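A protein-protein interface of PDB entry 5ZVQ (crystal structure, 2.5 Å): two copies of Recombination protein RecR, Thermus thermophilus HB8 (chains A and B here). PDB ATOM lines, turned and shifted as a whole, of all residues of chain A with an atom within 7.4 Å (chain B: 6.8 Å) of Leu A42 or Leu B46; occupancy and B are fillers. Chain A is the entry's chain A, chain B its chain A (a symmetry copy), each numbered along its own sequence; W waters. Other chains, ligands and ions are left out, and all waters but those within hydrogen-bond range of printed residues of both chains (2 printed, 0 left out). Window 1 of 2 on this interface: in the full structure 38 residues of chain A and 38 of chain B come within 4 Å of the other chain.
Leu A10 touches Leu B46, and with the chains exchanged Leu A46 touches Leu B10. Leu A32 touches Leu B46, and with the chains exchanged Leu A46 touches Leu B32. Ala A43 touches Leu B46, and with the chains exchanged Leu A46 touches Ala B43. Leu B46 touches its own counterpart, Leu A46. Positions printed for both chains: 9, 10, 13, 14, 32, 39, 40, 41, 42, 43, 44, 45, 46, 47 and 48. Of the 25 pairs that touch across the chains among the printed residues, 15 have their exchanged pair printed and touching as well.
Water W2 lies within hydrogen-bond range of O of Ala B45 and O of Ser A6. Water W1 lies within hydrogen-bond range of O of Ala B13 and OE2 of Glu A38.
Among the printed residues, pairs that only touch across the chains: Ser A6 with Gly B48, Ser A6 with Arg B51, Lys A9 with Ala B45, Leu A10 with Ala B45, Leu A10 with Leu B46, Leu A10 with Ile B49, Ala A13 with Leu B42, Leu A28 with Leu B17, Leu A32 with Leu B17, Leu A32 with Leu B46, Ala A33 with Ile B49, Lys A36 with Lys B50, Glu A38 with Leu B17, Leu A42 with Ala B13, Leu A42 with Leu B46, Ala A43 with Leu B46, Ala A45 with Lys B9, Ala A45 with Leu B10, Leu A46 with Leu B10, Leu A46 with Leu B32, Leu A46 with Leu B42, Leu A46 with Ala B43 and Leu A46 with Leu B46.
The side-chain amino group (NZ) of Lys A36 is in hydrogen-bond range of the backbone carbonyl oxygen (O) of Ile B49 (3.2 Å). OE2 of Glu A38 lies close to O of Arg B16, at 3.2 Å.
Hydrophobic or aromatic side chains of chain A within 4 Å of the printed part of chain B: Leu A10, Ala A13, Leu A28, Leu A32, Ala A33, Leu A42, Ala A45 and Leu A46. Of the 20 printed residues of chain B, 14 touch a printed residue of chain A. Hydrophobic or aromatic side chains of chain B within 4 Å of the printed part of chain A: Leu B10, Ala B13, Leu B17, Leu B32, Leu B42, Ala B45, Leu B46 and Ile B49. Among the printed residues, no Asp or Glu carboxylate lies within 4 Å of a Lys or Arg side-chain nitrogen of the other chain.
Of the printed residues of chain B, Leu A42 touches Ala B13 (3.8 Å) and Leu B46 (3.7 Å). Printed residues of chain A within 4 Å of Leu B46: Leu A10 (3.9 Å), Leu A32 (3.8 Å), Leu A42 (3.7 Å), Ala A43 (3.99 Å) and Leu A46 (3.4 Å). Of the printed residues of chain A, Arg B16 touches Glu A38. Of the printed residues of chain B, Leu A32 touches Leu B17 and Leu B46. Printed residues of chain A within 4 Å of Lys B50: Lys A36. Glu A37 touches none of the printed residues of chain B. Glu A47 touches none of the printed residues of chain B. The nearest printed residue of chain B that does not touch Leu A42 is Leu B14 (4.01 Å).
The backbone carbonyl oxygen (O) of Ala A33 is in hydrogen-bond range of the side-chain amino group (NZ) of Lys A36, 3.0 Å away. NE of Arg B51 lies within hydrogen-bond range of O of Gly B48, 2.7 Å away.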
ATOM      1  N   SER A   6      17.683 -16.265  -2.690  1.00  0.00           N
ATOM      2  CA  SER A   6      17.438 -16.267  -4.138  1.00  0.00           C
ATOM      3  C   SER A   6      16.240 -17.140  -4.523  1.00  0.00           C
ATOM      4  O   SER A   6      15.486 -16.798  -5.440  1.00  0.00           O
ATOM      5  CB  SER A   6      18.685 -16.732  -4.887  1.00  0.00           C
ATOM      6  OG  SER A   6      19.157 -17.947  -4.346  1.00  0.00           O
ATOM      7  N   LYS A   9      13.319 -15.037  -3.305  1.00  0.00           N
ATOM      8  CA  LYS A   9      13.258 -13.942  -4.279  1.00  0.00           C
ATOM      9  C   LYS A   9      12.580 -14.372  -5.588  1.00  0.00           C
ATOM     10  O   LYS A   9      11.816 -13.603  -6.168  1.00  0.00           O
ATOM     11  CB  LYS A   9      14.676 -13.420  -4.567  1.00  0.00           C
ATOM     12  CG  LYS A   9      14.751 -12.216  -5.497  1.00  0.00           C
ATOM     13  N   LEU A  10      12.869 -15.594  -6.041  1.00  0.00           N
ATOM     14  CA  LEU A  10      12.250 -16.162  -7.240  1.00  0.00           C
ATOM     15  C   LEU A  10      10.788 -16.513  -6.988  1.00  0.00           C
ATOM     16  O   LEU A  10       9.912 -16.143  -7.776  1.00  0.00           O
ATOM     17  CB  LEU A  10      13.012 -17.417  -7.694  1.00  0.00           C
ATOM     18  CG  LEU A  10      12.533 -18.149  -8.957  1.00  0.00           C
ATOM     19  CD1 LEU A  10      12.519 -17.210 -10.154  1.00  0.00           C
ATOM     20  CD2 LEU A  10      13.407 -19.361  -9.231  1.00  0.00           C
ATOM     21  N   ALA A  13       8.727 -13.364  -6.816  1.00  0.00           N
ATOM     22  CA  ALA A  13       8.536 -12.845  -8.173  1.00  0.00           C
ATOM     23  C   ALA A  13       7.516 -13.668  -8.953  1.00  0.00           C
ATOM     24  O   ALA A  13       6.658 -13.106  -9.628  1.00  0.00           O
ATOM     25  CB  ALA A  13       9.861 -12.800  -8.922  1.00  0.00           C
ATOM     26  N   LEU A  14       7.610 -14.993  -8.856  1.00  0.00           N
ATOM     27  CA  LEU A  14       6.627 -15.885  -9.486  1.00  0.00           C
ATOM     28  C   LEU A  14       5.196 -15.680  -8.967  1.00  0.00           C
ATOM     29  O   LEU A  14       4.239 -15.871  -9.716  1.00  0.00           O
ATOM     30  CB  LEU A  14       7.036 -17.354  -9.328  1.00  0.00           C
ATOM     31  CG  LEU A  14       8.232 -17.828 -10.167  1.00  0.00           C
ATOM     32  CD1 LEU A  14       8.721 -19.188  -9.687  1.00  0.00           C
ATOM     33  CD2 LEU A  14       7.891 -17.879 -11.649  1.00  0.00           C
ATOM     34  N   LEU A  28       7.355 -24.304  -8.931  1.00  0.00           N
ATOM     35  CA  LEU A  28       8.058 -23.800 -10.109  1.00  0.00           C
ATOM     36  C   LEU A  28       9.449 -23.295  -9.764  1.00  0.00           C
ATOM     37  O   LEU A  28      10.391 -23.524 -10.521  1.00  0.00           O
ATOM     38  CB  LEU A  28       7.256 -22.674 -10.767  1.00  0.00           C
ATOM     39  CG  LEU A  28       5.904 -23.087 -11.358  1.00  0.00           C
ATOM     40  CD1 LEU A  28       5.133 -21.851 -11.797  1.00  0.00           C
ATOM     41  CD2 LEU A  28       6.078 -24.067 -12.510  1.00  0.00           C
ATOM     42  N   ALA A  29       9.557 -22.595  -8.633  1.00  0.00           N
ATOM     43  CA  ALA A  29      10.833 -22.089  -8.126  1.00  0.00           C
ATOM     44  C   ALA A  29      11.807 -23.229  -7.848  1.00  0.00           C
ATOM     45  O   ALA A  29      12.974 -23.160  -8.244  1.00  0.00           O
ATOM     46  CB  ALA A  29      10.612 -21.265  -6.866  1.00  0.00           C
ATOM     47  N   LEU A  32      12.878 -24.729 -11.191  1.00  0.00           N
ATOM     48  CA  LEU A  32      13.860 -23.880 -11.880  1.00  0.00           C
ATOM     49  C   LEU A  32      15.242 -24.002 -11.242  1.00  0.00           C
ATOM     50  O   LEU A  32      16.242 -24.068 -11.954  1.00  0.00           O
ATOM     51  CB  LEU A  32      13.402 -22.414 -11.930  1.00  0.00           C
ATOM     52  CG  LEU A  32      12.214 -22.145 -12.869  1.00  0.00           C
ATOM     53  CD1 LEU A  32      11.552 -20.800 -12.570  1.00  0.00           C
ATOM     54  CD2 LEU A  32      12.635 -22.234 -14.331  1.00  0.00           C
ATOM     55  N   ALA A  33      15.287 -24.067  -9.911  1.00  0.00           N
ATOM     56  CA  ALA A  33      16.538 -24.306  -9.183  1.00  0.00           C
ATOM     57  C   ALA A  33      17.199 -25.644  -9.550  1.00  0.00           C
ATOM     58  O   ALA A  33      18.420 -25.710  -9.669  1.00  0.00           O
ATOM     59  CB  ALA A  33      16.301 -24.228  -7.684  1.00  0.00           C
ATOM     60  N   LYS A  36      18.947 -25.892 -14.155  1.00  0.00           N
ATOM     61  CA  LYS A  36      19.730 -24.682 -14.474  1.00  0.00           C
ATOM     62  C   LYS A  36      19.618 -24.251 -15.935  1.00  0.00           C
ATOM     63  O   LYS A  36      19.491 -23.054 -16.218  1.00  0.00           O
ATOM     64  CB  LYS A  36      21.219 -24.850 -14.106  1.00  0.00           C
ATOM     65  CG  LYS A  36      21.668 -24.046 -12.892  1.00  0.00           C
ATOM     66  CD  LYS A  36      20.993 -24.494 -11.604  1.00  0.00           C
ATOM     67  CE  LYS A  36      21.533 -23.721 -10.408  1.00  0.00           C
ATOM     68  NZ  LYS A  36      20.687 -23.866  -9.193  1.00  0.00           N
ATOM     69  N   GLU A  37      19.677 -25.227 -16.847  1.00  0.00           N
ATOM     70  CA  GLU A  37      19.609 -24.958 -18.287  1.00  0.00           C
ATOM     71  C   GLU A  37      18.298 -24.265 -18.654  1.00  0.00           C
ATOM     72  O   GLU A  37      18.310 -23.214 -19.295  1.00  0.00           O
ATOM     73  CB  GLU A  37      19.772 -26.251 -19.098  1.00  0.00           C
ATOM     74  N   GLU A  38      17.186 -24.848 -18.212  1.00  0.00           N
ATOM     75  CA  GLU A  38      15.853 -24.300 -18.465  1.00  0.00           C
ATOM     76  C   GLU A  38      15.683 -22.889 -17.875  1.00  0.00           C
ATOM     77  O   GLU A  38      15.110 -22.010 -18.524  1.00  0.00           O
ATOM     78  CB  GLU A  38      14.775 -25.258 -17.922  1.00  0.00           C
ATOM     79  CG  GLU A  38      13.340 -24.894 -18.288  1.00  0.00           C
ATOM     80  CD  GLU A  38      12.303 -25.868 -17.738  1.00  0.00           C
ATOM     81  OE1 GLU A  38      12.676 -26.960 -17.264  1.00  0.00           O
ATOM     82  OE2 GLU A  38      11.098 -25.541 -17.784  1.00  0.00           O
ATOM     83  N   ALA A  39      16.192 -22.673 -16.662  1.00  0.00           N
ATOM     84  CA  ALA A  39      16.101 -21.365 -16.005  1.00  0.00           C
ATOM     85  C   ALA A  39      16.876 -20.280 -16.752  1.00  0.00           C
ATOM     86  O   ALA A  39      16.407 -19.143 -16.853  1.00  0.00           O
ATOM     87  CB  ALA A  39      16.577 -21.453 -14.562  1.00  0.00           C
ATOM     88  N   GLU A  40      18.056 -20.628 -17.264  1.00  0.00           N
ATOM     89  CA  GLU A  40      18.850 -19.711 -18.094  1.00  0.00           C
ATOM     90  C   GLU A  40      18.094 -19.332 -19.371  1.00  0.00           C
ATOM     91  O   GLU A  40      18.031 -18.152 -19.735  1.00  0.00           O
ATOM     92  CB  GLU A  40      20.210 -20.325 -18.449  1.00  0.00           C
ATOM     93  N   ALA A  41      17.509 -20.332 -20.029  1.00  0.00           N
ATOM     94  CA  ALA A  41      16.677 -20.115 -21.222  1.00  0.00           C
ATOM     95  C   ALA A  41      15.485 -19.177 -20.969  1.00  0.00           C
ATOM     96  O   ALA A  41      15.141 -18.367 -21.840  1.00  0.00           O
ATOM     97  CB  ALA A  41      16.191 -21.442 -21.783  1.00  0.00           C
ATOM     98  N   LEU A  42      14.874 -19.283 -19.787  1.00  0.00           N
ATOM     99  CA  LEU A  42      13.755 -18.410 -19.408  1.00  0.00           C
ATOM    100  C   LEU A  42      14.212 -16.982 -19.149  1.00  0.00           C
ATOM    101  O   LEU A  42      13.531 -16.031 -19.540  1.00  0.00           O
ATOM    102  CB  LEU A  42      13.025 -18.949 -18.175  1.00  0.00           C
ATOM    103  CG  LEU A  42      11.753 -18.208 -17.744  1.00  0.00           C
ATOM    104  CD1 LEU A  42      10.708 -18.243 -18.845  1.00  0.00           C
ATOM    105  CD2 LEU A  42      11.200 -18.810 -16.462  1.00  0.00           C
ATOM    106  N   ALA A  43      15.352 -16.843 -18.478  1.00  0.00           N
ATOM    107  CA  ALA A  43      16.002 -15.537 -18.286  1.00  0.00           C
ATOM    108  C   ALA A  43      16.425 -14.888 -19.608  1.00  0.00           C
ATOM    109  O   ALA A  43      16.337 -13.670 -19.754  1.00  0.00           O
ATOM    110  CB  ALA A  43      17.209 -15.681 -17.373  1.00  0.00           C
ATOM    111  N   GLU A  44      16.890 -15.703 -20.552  1.00  0.00           N
ATOM    112  CA  GLU A  44      17.248 -15.223 -21.885  1.00  0.00           C
ATOM    113  C   GLU A  44      16.016 -14.681 -22.617  1.00  0.00           C
ATOM    114  O   GLU A  44      16.055 -13.581 -23.179  1.00  0.00           O
ATOM    115  CB  GLU A  44      17.899 -16.345 -22.702  1.00  0.00           C
ATOM    116  CG  GLU A  44      18.508 -15.881 -24.020  1.00  0.00           C
ATOM    117  CD  GLU A  44      19.373 -16.939 -24.687  1.00  0.00           C
ATOM    118  OE1 GLU A  44      20.274 -17.494 -24.016  1.00  0.00           O
ATOM    119  OE2 GLU A  44      19.162 -17.204 -25.893  1.00  0.00           O
ATOM    120  N   ALA A  45      14.929 -15.458 -22.584  1.00  0.00           N
ATOM    121  CA  ALA A  45      13.650 -15.068 -23.181  1.00  0.00           C
ATOM    122  C   ALA A  45      13.026 -13.831 -22.529  1.00  0.00           C
ATOM    123  O   ALA A  45      12.394 -13.022 -23.213  1.00  0.00           O
ATOM    124  CB  ALA A  45      12.675 -16.228 -23.120  1.00  0.00           C
ATOM    125  N   LEU A  46      13.192 -13.697 -21.212  1.00  0.00           N
ATOM    126  CA  LEU A  46      12.714 -12.515 -20.487  1.00  0.00           C
ATOM    127  C   LEU A  46      13.495 -11.262 -20.863  1.00  0.00           C
ATOM    128  O   LEU A  46      12.903 -10.199 -21.049  1.00  0.00           O
ATOM    129  CB  LEU A  46      12.773 -12.732 -18.973  1.00  0.00           C
ATOM    130  CG  LEU A  46      11.627 -13.585 -18.426  1.00  0.00           C
ATOM    131  CD1 LEU A  46      11.991 -14.172 -17.072  1.00  0.00           C
ATOM    132  CD2 LEU A  46      10.335 -12.779 -18.340  1.00  0.00           C
ATOM    133  N   GLU A  47      14.818 -11.386 -20.955  1.00  0.00           N
ATOM    134  CA  GLU A  47      15.653 -10.313 -21.517  1.00  0.00           C
ATOM    135  C   GLU A  47      15.248 -10.038 -22.965  1.00  0.00           C
ATOM    136  O   GLU A  47      15.111  -8.882 -23.364  1.00  0.00           O
ATOM    137  CB  GLU A  47      17.155 -10.648 -21.437  1.00  0.00           C
ATOM    138  CG  GLU A  47      17.925  -9.827 -20.409  1.00  0.00           C
ATOM    139  CD  GLU A  47      18.018  -8.353 -20.776  1.00  0.00           C
ATOM    140  OE1 GLU A  47      18.016  -7.512 -19.852  1.00  0.00           O
ATOM    141  OE2 GLU A  47      18.084  -8.029 -21.984  1.00  0.00           O
ATOM    142  N   GLY A  48      15.040 -11.112 -23.727  1.00  0.00           N
ATOM    143  CA  GLY A  48      14.555 -11.037 -25.098  1.00  0.00           C
ATOM    144  C   GLY A  48      13.317 -10.180 -25.312  1.00  0.00           C
ATOM    145  O   GLY A  48      13.217  -9.512 -26.335  1.00  0.00           O
ATOM    146  N   LYS B   9       9.210 -17.018 -28.103  1.00  0.00           N
ATOM    147  CA  LYS B   9      10.354 -17.547 -27.354  1.00  0.00           C
ATOM    148  C   LYS B   9      10.073 -17.618 -25.846  1.00  0.00           C
ATOM    149  O   LYS B   9      10.470 -18.579 -25.190  1.00  0.00           O
ATOM    150  CB  LYS B   9      11.597 -16.679 -27.618  1.00  0.00           C
ATOM    151  CG  LYS B   9      12.885 -17.171 -26.971  1.00  0.00           C
ATOM    152  N   LEU B  10       9.397 -16.598 -25.313  1.00  0.00           N
ATOM    153  CA  LEU B  10       9.001 -16.560 -23.903  1.00  0.00           C
ATOM    154  C   LEU B  10       7.883 -17.557 -23.620  1.00  0.00           C
ATOM    155  O   LEU B  10       7.970 -18.339 -22.669  1.00  0.00           O
ATOM    156  CB  LEU B  10       8.544 -15.146 -23.513  1.00  0.00           C
ATOM    157  CG  LEU B  10       8.112 -14.889 -22.062  1.00  0.00           C
ATOM    158  CD1 LEU B  10       9.227 -15.253 -21.093  1.00  0.00           C
ATOM    159  CD2 LEU B  10       7.691 -13.441 -21.881  1.00  0.00           C
ATOM    160  N   ALA B  13       9.258 -21.064 -23.650  1.00  0.00           N
ATOM    161  CA  ALA B  13       9.998 -21.297 -22.408  1.00  0.00           C
ATOM    162  C   ALA B  13       9.061 -21.496 -21.221  1.00  0.00           C
ATOM    163  O   ALA B  13       9.274 -22.395 -20.412  1.00  0.00           O
ATOM    164  CB  ALA B  13      10.959 -20.147 -22.132  1.00  0.00           C
ATOM    165  N   LEU B  14       8.027 -20.662 -21.123  1.00  0.00           N
ATOM    166  CA  LEU B  14       7.006 -20.816 -20.077  1.00  0.00           C
ATOM    167  C   LEU B  14       6.262 -22.158 -20.145  1.00  0.00           C
ATOM    168  O   LEU B  14       5.848 -22.683 -19.112  1.00  0.00           O
ATOM    169  CB  LEU B  14       6.003 -19.658 -20.112  1.00  0.00           C
ATOM    170  CG  LEU B  14       6.513 -18.293 -19.627  1.00  0.00           C
ATOM    171  CD1 LEU B  14       5.536 -17.188 -20.006  1.00  0.00           C
ATOM    172  CD2 LEU B  14       6.763 -18.290 -18.126  1.00  0.00           C
ATOM    173  N   ARG B  16       7.568 -25.085 -21.045  1.00  0.00           N
ATOM    174  CA  ARG B  16       8.439 -26.128 -20.475  1.00  0.00           C
ATOM    175  C   ARG B  16       8.231 -26.362 -18.968  1.00  0.00           C
ATOM    176  O   ARG B  16       8.633 -27.406 -18.452  1.00  0.00           O
ATOM    177  CB  ARG B  16       9.914 -25.795 -20.708  1.00  0.00           C
ATOM    178  CG  ARG B  16      10.361 -25.829 -22.158  1.00  0.00           C
ATOM    179  CD  ARG B  16      11.853 -25.539 -22.271  1.00  0.00           C
ATOM    180  NE  ARG B  16      12.676 -26.543 -21.585  1.00  0.00           N
ATOM    181  CZ  ARG B  16      14.005 -26.491 -21.470  1.00  0.00           C
ATOM    182  NH1 ARG B  16      14.709 -25.484 -21.992  1.00  0.00           N
ATOM    183  NH2 ARG B  16      14.644 -27.461 -20.822  1.00  0.00           N
ATOM    184  N   LEU B  17       7.631 -25.394 -18.269  1.00  0.00           N
ATOM    185  CA  LEU B  17       7.377 -25.508 -16.835  1.00  0.00           C
ATOM    186  C   LEU B  17       6.273 -26.540 -16.547  1.00  0.00           C
ATOM    187  O   LEU B  17       5.275 -26.585 -17.267  1.00  0.00           O
ATOM    188  CB  LEU B  17       6.969 -24.148 -16.261  1.00  0.00           C
ATOM    189  CG  LEU B  17       7.964 -22.989 -16.401  1.00  0.00           C
ATOM    190  CD1 LEU B  17       7.351 -21.686 -15.908  1.00  0.00           C
ATOM    191  CD2 LEU B  17       9.262 -23.282 -15.663  1.00  0.00           C
ATOM    192  N   LEU B  32       3.772 -10.397 -18.999  1.00  0.00           N
ATOM    193  CA  LEU B  32       5.173 -10.000 -18.803  1.00  0.00           C
ATOM    194  C   LEU B  32       5.594  -8.937 -19.815  1.00  0.00           C
ATOM    195  O   LEU B  32       6.286  -7.987 -19.454  1.00  0.00           O
ATOM    196  CB  LEU B  32       6.115 -11.214 -18.854  1.00  0.00           C
ATOM    197  CG  LEU B  32       6.007 -12.160 -17.646  1.00  0.00           C
ATOM    198  CD1 LEU B  32       6.636 -13.522 -17.938  1.00  0.00           C
ATOM    199  CD2 LEU B  32       6.616 -11.533 -16.398  1.00  0.00           C
ATOM    200  N   ALA B  39       8.851  -8.068 -15.268  1.00  0.00           N
ATOM    201  CA  ALA B  39       9.636  -9.014 -16.069  1.00  0.00           C
ATOM    202  C   ALA B  39      11.136  -8.911 -15.794  1.00  0.00           C
ATOM    203  O   ALA B  39      11.827  -9.932 -15.739  1.00  0.00           O
ATOM    204  CB  ALA B  39       9.358  -8.822 -17.554  1.00  0.00           C
ATOM    205  N   GLU B  40      11.634  -7.686 -15.630  1.00  0.00           N
ATOM    206  CA  GLU B  40      13.037  -7.456 -15.256  1.00  0.00           C
ATOM    207  C   GLU B  40      13.348  -8.067 -13.886  1.00  0.00           C
ATOM    208  O   GLU B  40      14.366  -8.748 -13.720  1.00  0.00           O
ATOM    209  CB  GLU B  40      13.368  -5.958 -15.251  1.00  0.00           C
ATOM    210  N   ALA B  41      12.456  -7.838 -12.922  1.00  0.00           N
ATOM    211  CA  ALA B  41      12.573  -8.429 -11.581  1.00  0.00           C
ATOM    212  C   ALA B  41      12.618  -9.966 -11.596  1.00  0.00           C
ATOM    213  O   ALA B  41      13.356 -10.570 -10.807  1.00  0.00           O
ATOM    214  CB  ALA B  41      11.443  -7.946 -10.685  1.00  0.00           C
ATOM    215  N   LEU B  42      11.843 -10.584 -12.491  1.00  0.00           N
ATOM    216  CA  LEU B  42      11.836 -12.046 -12.635  1.00  0.00           C
ATOM    217  C   LEU B  42      13.125 -12.561 -13.257  1.00  0.00           C
ATOM    218  O   LEU B  42      13.649 -13.594 -12.834  1.00  0.00           O
ATOM    219  CB  LEU B  42      10.639 -12.512 -13.469  1.00  0.00           C
ATOM    220  CG  LEU B  42      10.430 -14.027 -13.593  1.00  0.00           C
ATOM    221  CD1 LEU B  42      10.206 -14.655 -12.229  1.00  0.00           C
ATOM    222  CD2 LEU B  42       9.261 -14.325 -14.517  1.00  0.00           C
ATOM    223  N   ALA B  43      13.616 -11.848 -14.267  1.00  0.00           N
ATOM    224  CA  ALA B  43      14.930 -12.127 -14.866  1.00  0.00           C
ATOM    225  C   ALA B  43      16.082 -11.954 -13.871  1.00  0.00           C
ATOM    226  O   ALA B  43      17.050 -12.713 -13.906  1.00  0.00           O
ATOM    227  CB  ALA B  43      15.156 -11.235 -16.076  1.00  0.00           C
ATOM    228  N   GLU B  44      15.975 -10.953 -13.001  1.00  0.00           N
ATOM    229  CA  GLU B  44      16.962 -10.730 -11.946  1.00  0.00           C
ATOM    230  C   GLU B  44      16.983 -11.905 -10.963  1.00  0.00           C
ATOM    231  O   GLU B  44      18.054 -12.424 -10.631  1.00  0.00           O
ATOM    232  CB  GLU B  44      16.667  -9.422 -11.204  1.00  0.00           C
ATOM    233  CG  GLU B  44      17.768  -8.993 -10.240  1.00  0.00           C
ATOM    234  CD  GLU B  44      17.588  -7.576  -9.715  1.00  0.00           C
ATOM    235  OE1 GLU B  44      17.404  -6.647 -10.535  1.00  0.00           O
ATOM    236  OE2 GLU B  44      17.648  -7.391  -8.478  1.00  0.00           O
ATOM    237  N   ALA B  45      15.791 -12.318 -10.524  1.00  0.00           N
ATOM    238  CA  ALA B  45      15.623 -13.463  -9.627  1.00  0.00           C
ATOM    239  C   ALA B  45      16.076 -14.790 -10.243  1.00  0.00           C
ATOM    240  O   ALA B  45      16.605 -15.653  -9.538  1.00  0.00           O
ATOM    241  CB  ALA B  45      14.176 -13.569  -9.185  1.00  0.00           C
ATOM    242  N   LEU B  46      15.853 -14.954 -11.548  1.00  0.00           N
ATOM    243  CA  LEU B  46      16.315 -16.144 -12.269  1.00  0.00           C
ATOM    244  C   LEU B  46      17.834 -16.196 -12.371  1.00  0.00           C
ATOM    245  O   LEU B  46      18.429 -17.257 -12.185  1.00  0.00           O
ATOM    246  CB  LEU B  46      15.695 -16.219 -13.668  1.00  0.00           C
ATOM    247  CG  LEU B  46      14.251 -16.720 -13.677  1.00  0.00           C
ATOM    248  CD1 LEU B  46      13.547 -16.311 -14.961  1.00  0.00           C
ATOM    249  CD2 LEU B  46      14.191 -18.232 -13.483  1.00  0.00           C
ATOM    250  N   GLU B  47      18.452 -15.057 -12.682  1.00  0.00           N
ATOM    251  CA  GLU B  47      19.915 -14.930 -12.596  1.00  0.00           C
ATOM    252  C   GLU B  47      20.380 -15.174 -11.161  1.00  0.00           C
ATOM    253  O   GLU B  47      21.352 -15.894 -10.934  1.00  0.00           O
ATOM    254  CB  GLU B  47      20.405 -13.555 -13.090  1.00  0.00           C
ATOM    255  CG  GLU B  47      21.132 -13.593 -14.428  1.00  0.00           C
ATOM    256  CD  GLU B  47      22.467 -14.322 -14.357  1.00  0.00           C
ATOM    257  OE1 GLU B  47      22.843 -14.968 -15.359  1.00  0.00           O
ATOM    258  OE2 GLU B  47      23.139 -14.260 -13.303  1.00  0.00           O
ATOM    259  N   GLY B  48      19.659 -14.585 -10.206  1.00  0.00           N
ATOM    260  CA  GLY B  48      19.899 -14.788  -8.784  1.00  0.00           C
ATOM    261  C   GLY B  48      20.003 -16.238  -8.334  1.00  0.00           C
ATOM    262  O   GLY B  48      20.804 -16.540  -7.457  1.00  0.00           O
ATOM    263  N   ILE B  49      19.213 -17.134  -8.934  1.00  0.00           N
ATOM    264  CA  ILE B  49      19.168 -18.546  -8.513  1.00  0.00           C
ATOM    265  C   ILE B  49      20.221 -19.449  -9.187  1.00  0.00           C
ATOM    266  O   ILE B  49      20.222 -20.662  -8.971  1.00  0.00           O
ATOM    267  CB  ILE B  49      17.724 -19.125  -8.657  1.00  0.00           C
ATOM    268  CG1 ILE B  49      17.437 -20.160  -7.563  1.00  0.00           C
ATOM    269  CG2 ILE B  49      17.458 -19.718 -10.041  1.00  0.00           C
ATOM    270  CD1 ILE B  49      15.970 -20.478  -7.405  1.00  0.00           C
ATOM    271  N   LYS B  50      21.111 -18.863  -9.990  1.00  0.00           N
ATOM    272  CA  LYS B  50      22.245 -19.590 -10.573  1.00  0.00           C
ATOM    273  C   LYS B  50      23.185 -20.110  -9.484  1.00  0.00           C
ATOM    274  O   LYS B  50      23.728 -21.212  -9.592  1.00  0.00           O
ATOM    275  CB  LYS B  50      23.021 -18.689 -11.542  1.00  0.00           C
ATOM    276  N   ARG B  51      23.364 -19.299  -8.443  1.00  0.00           N
ATOM    277  CA  ARG B  51      24.145 -19.671  -7.261  1.00  0.00           C
ATOM    278  C   ARG B  51      23.636 -20.916  -6.531  1.00  0.00           C
ATOM    279  O   ARG B  51      24.442 -21.749  -6.112  1.00  0.00           O
ATOM    280  CB  ARG B  51      24.219 -18.486  -6.276  1.00  0.00           C
ATOM    281  CG  ARG B  51      22.893 -18.107  -5.620  1.00  0.00           C
ATOM    282  CD  ARG B  51      22.871 -16.675  -5.090  1.00  0.00           C
ATOM    283  NE  ARG B  51      22.981 -15.656  -6.139  1.00  0.00           N
ATOM    284  CZ  ARG B  51      22.967 -14.334  -5.934  1.00  0.00           C
ATOM    285  NH1 ARG B  51      22.845 -13.827  -4.705  1.00  0.00           N
ATOM    286  NH2 ARG B  51      23.076 -13.505  -6.971  1.00  0.00           N
HETATM  287  O   HOH W   1      11.220 -22.418 -18.598  1.00  0.00           O
HETATM  288  O   HOH W   2      16.830 -15.222  -7.105  1.00  0.00           O
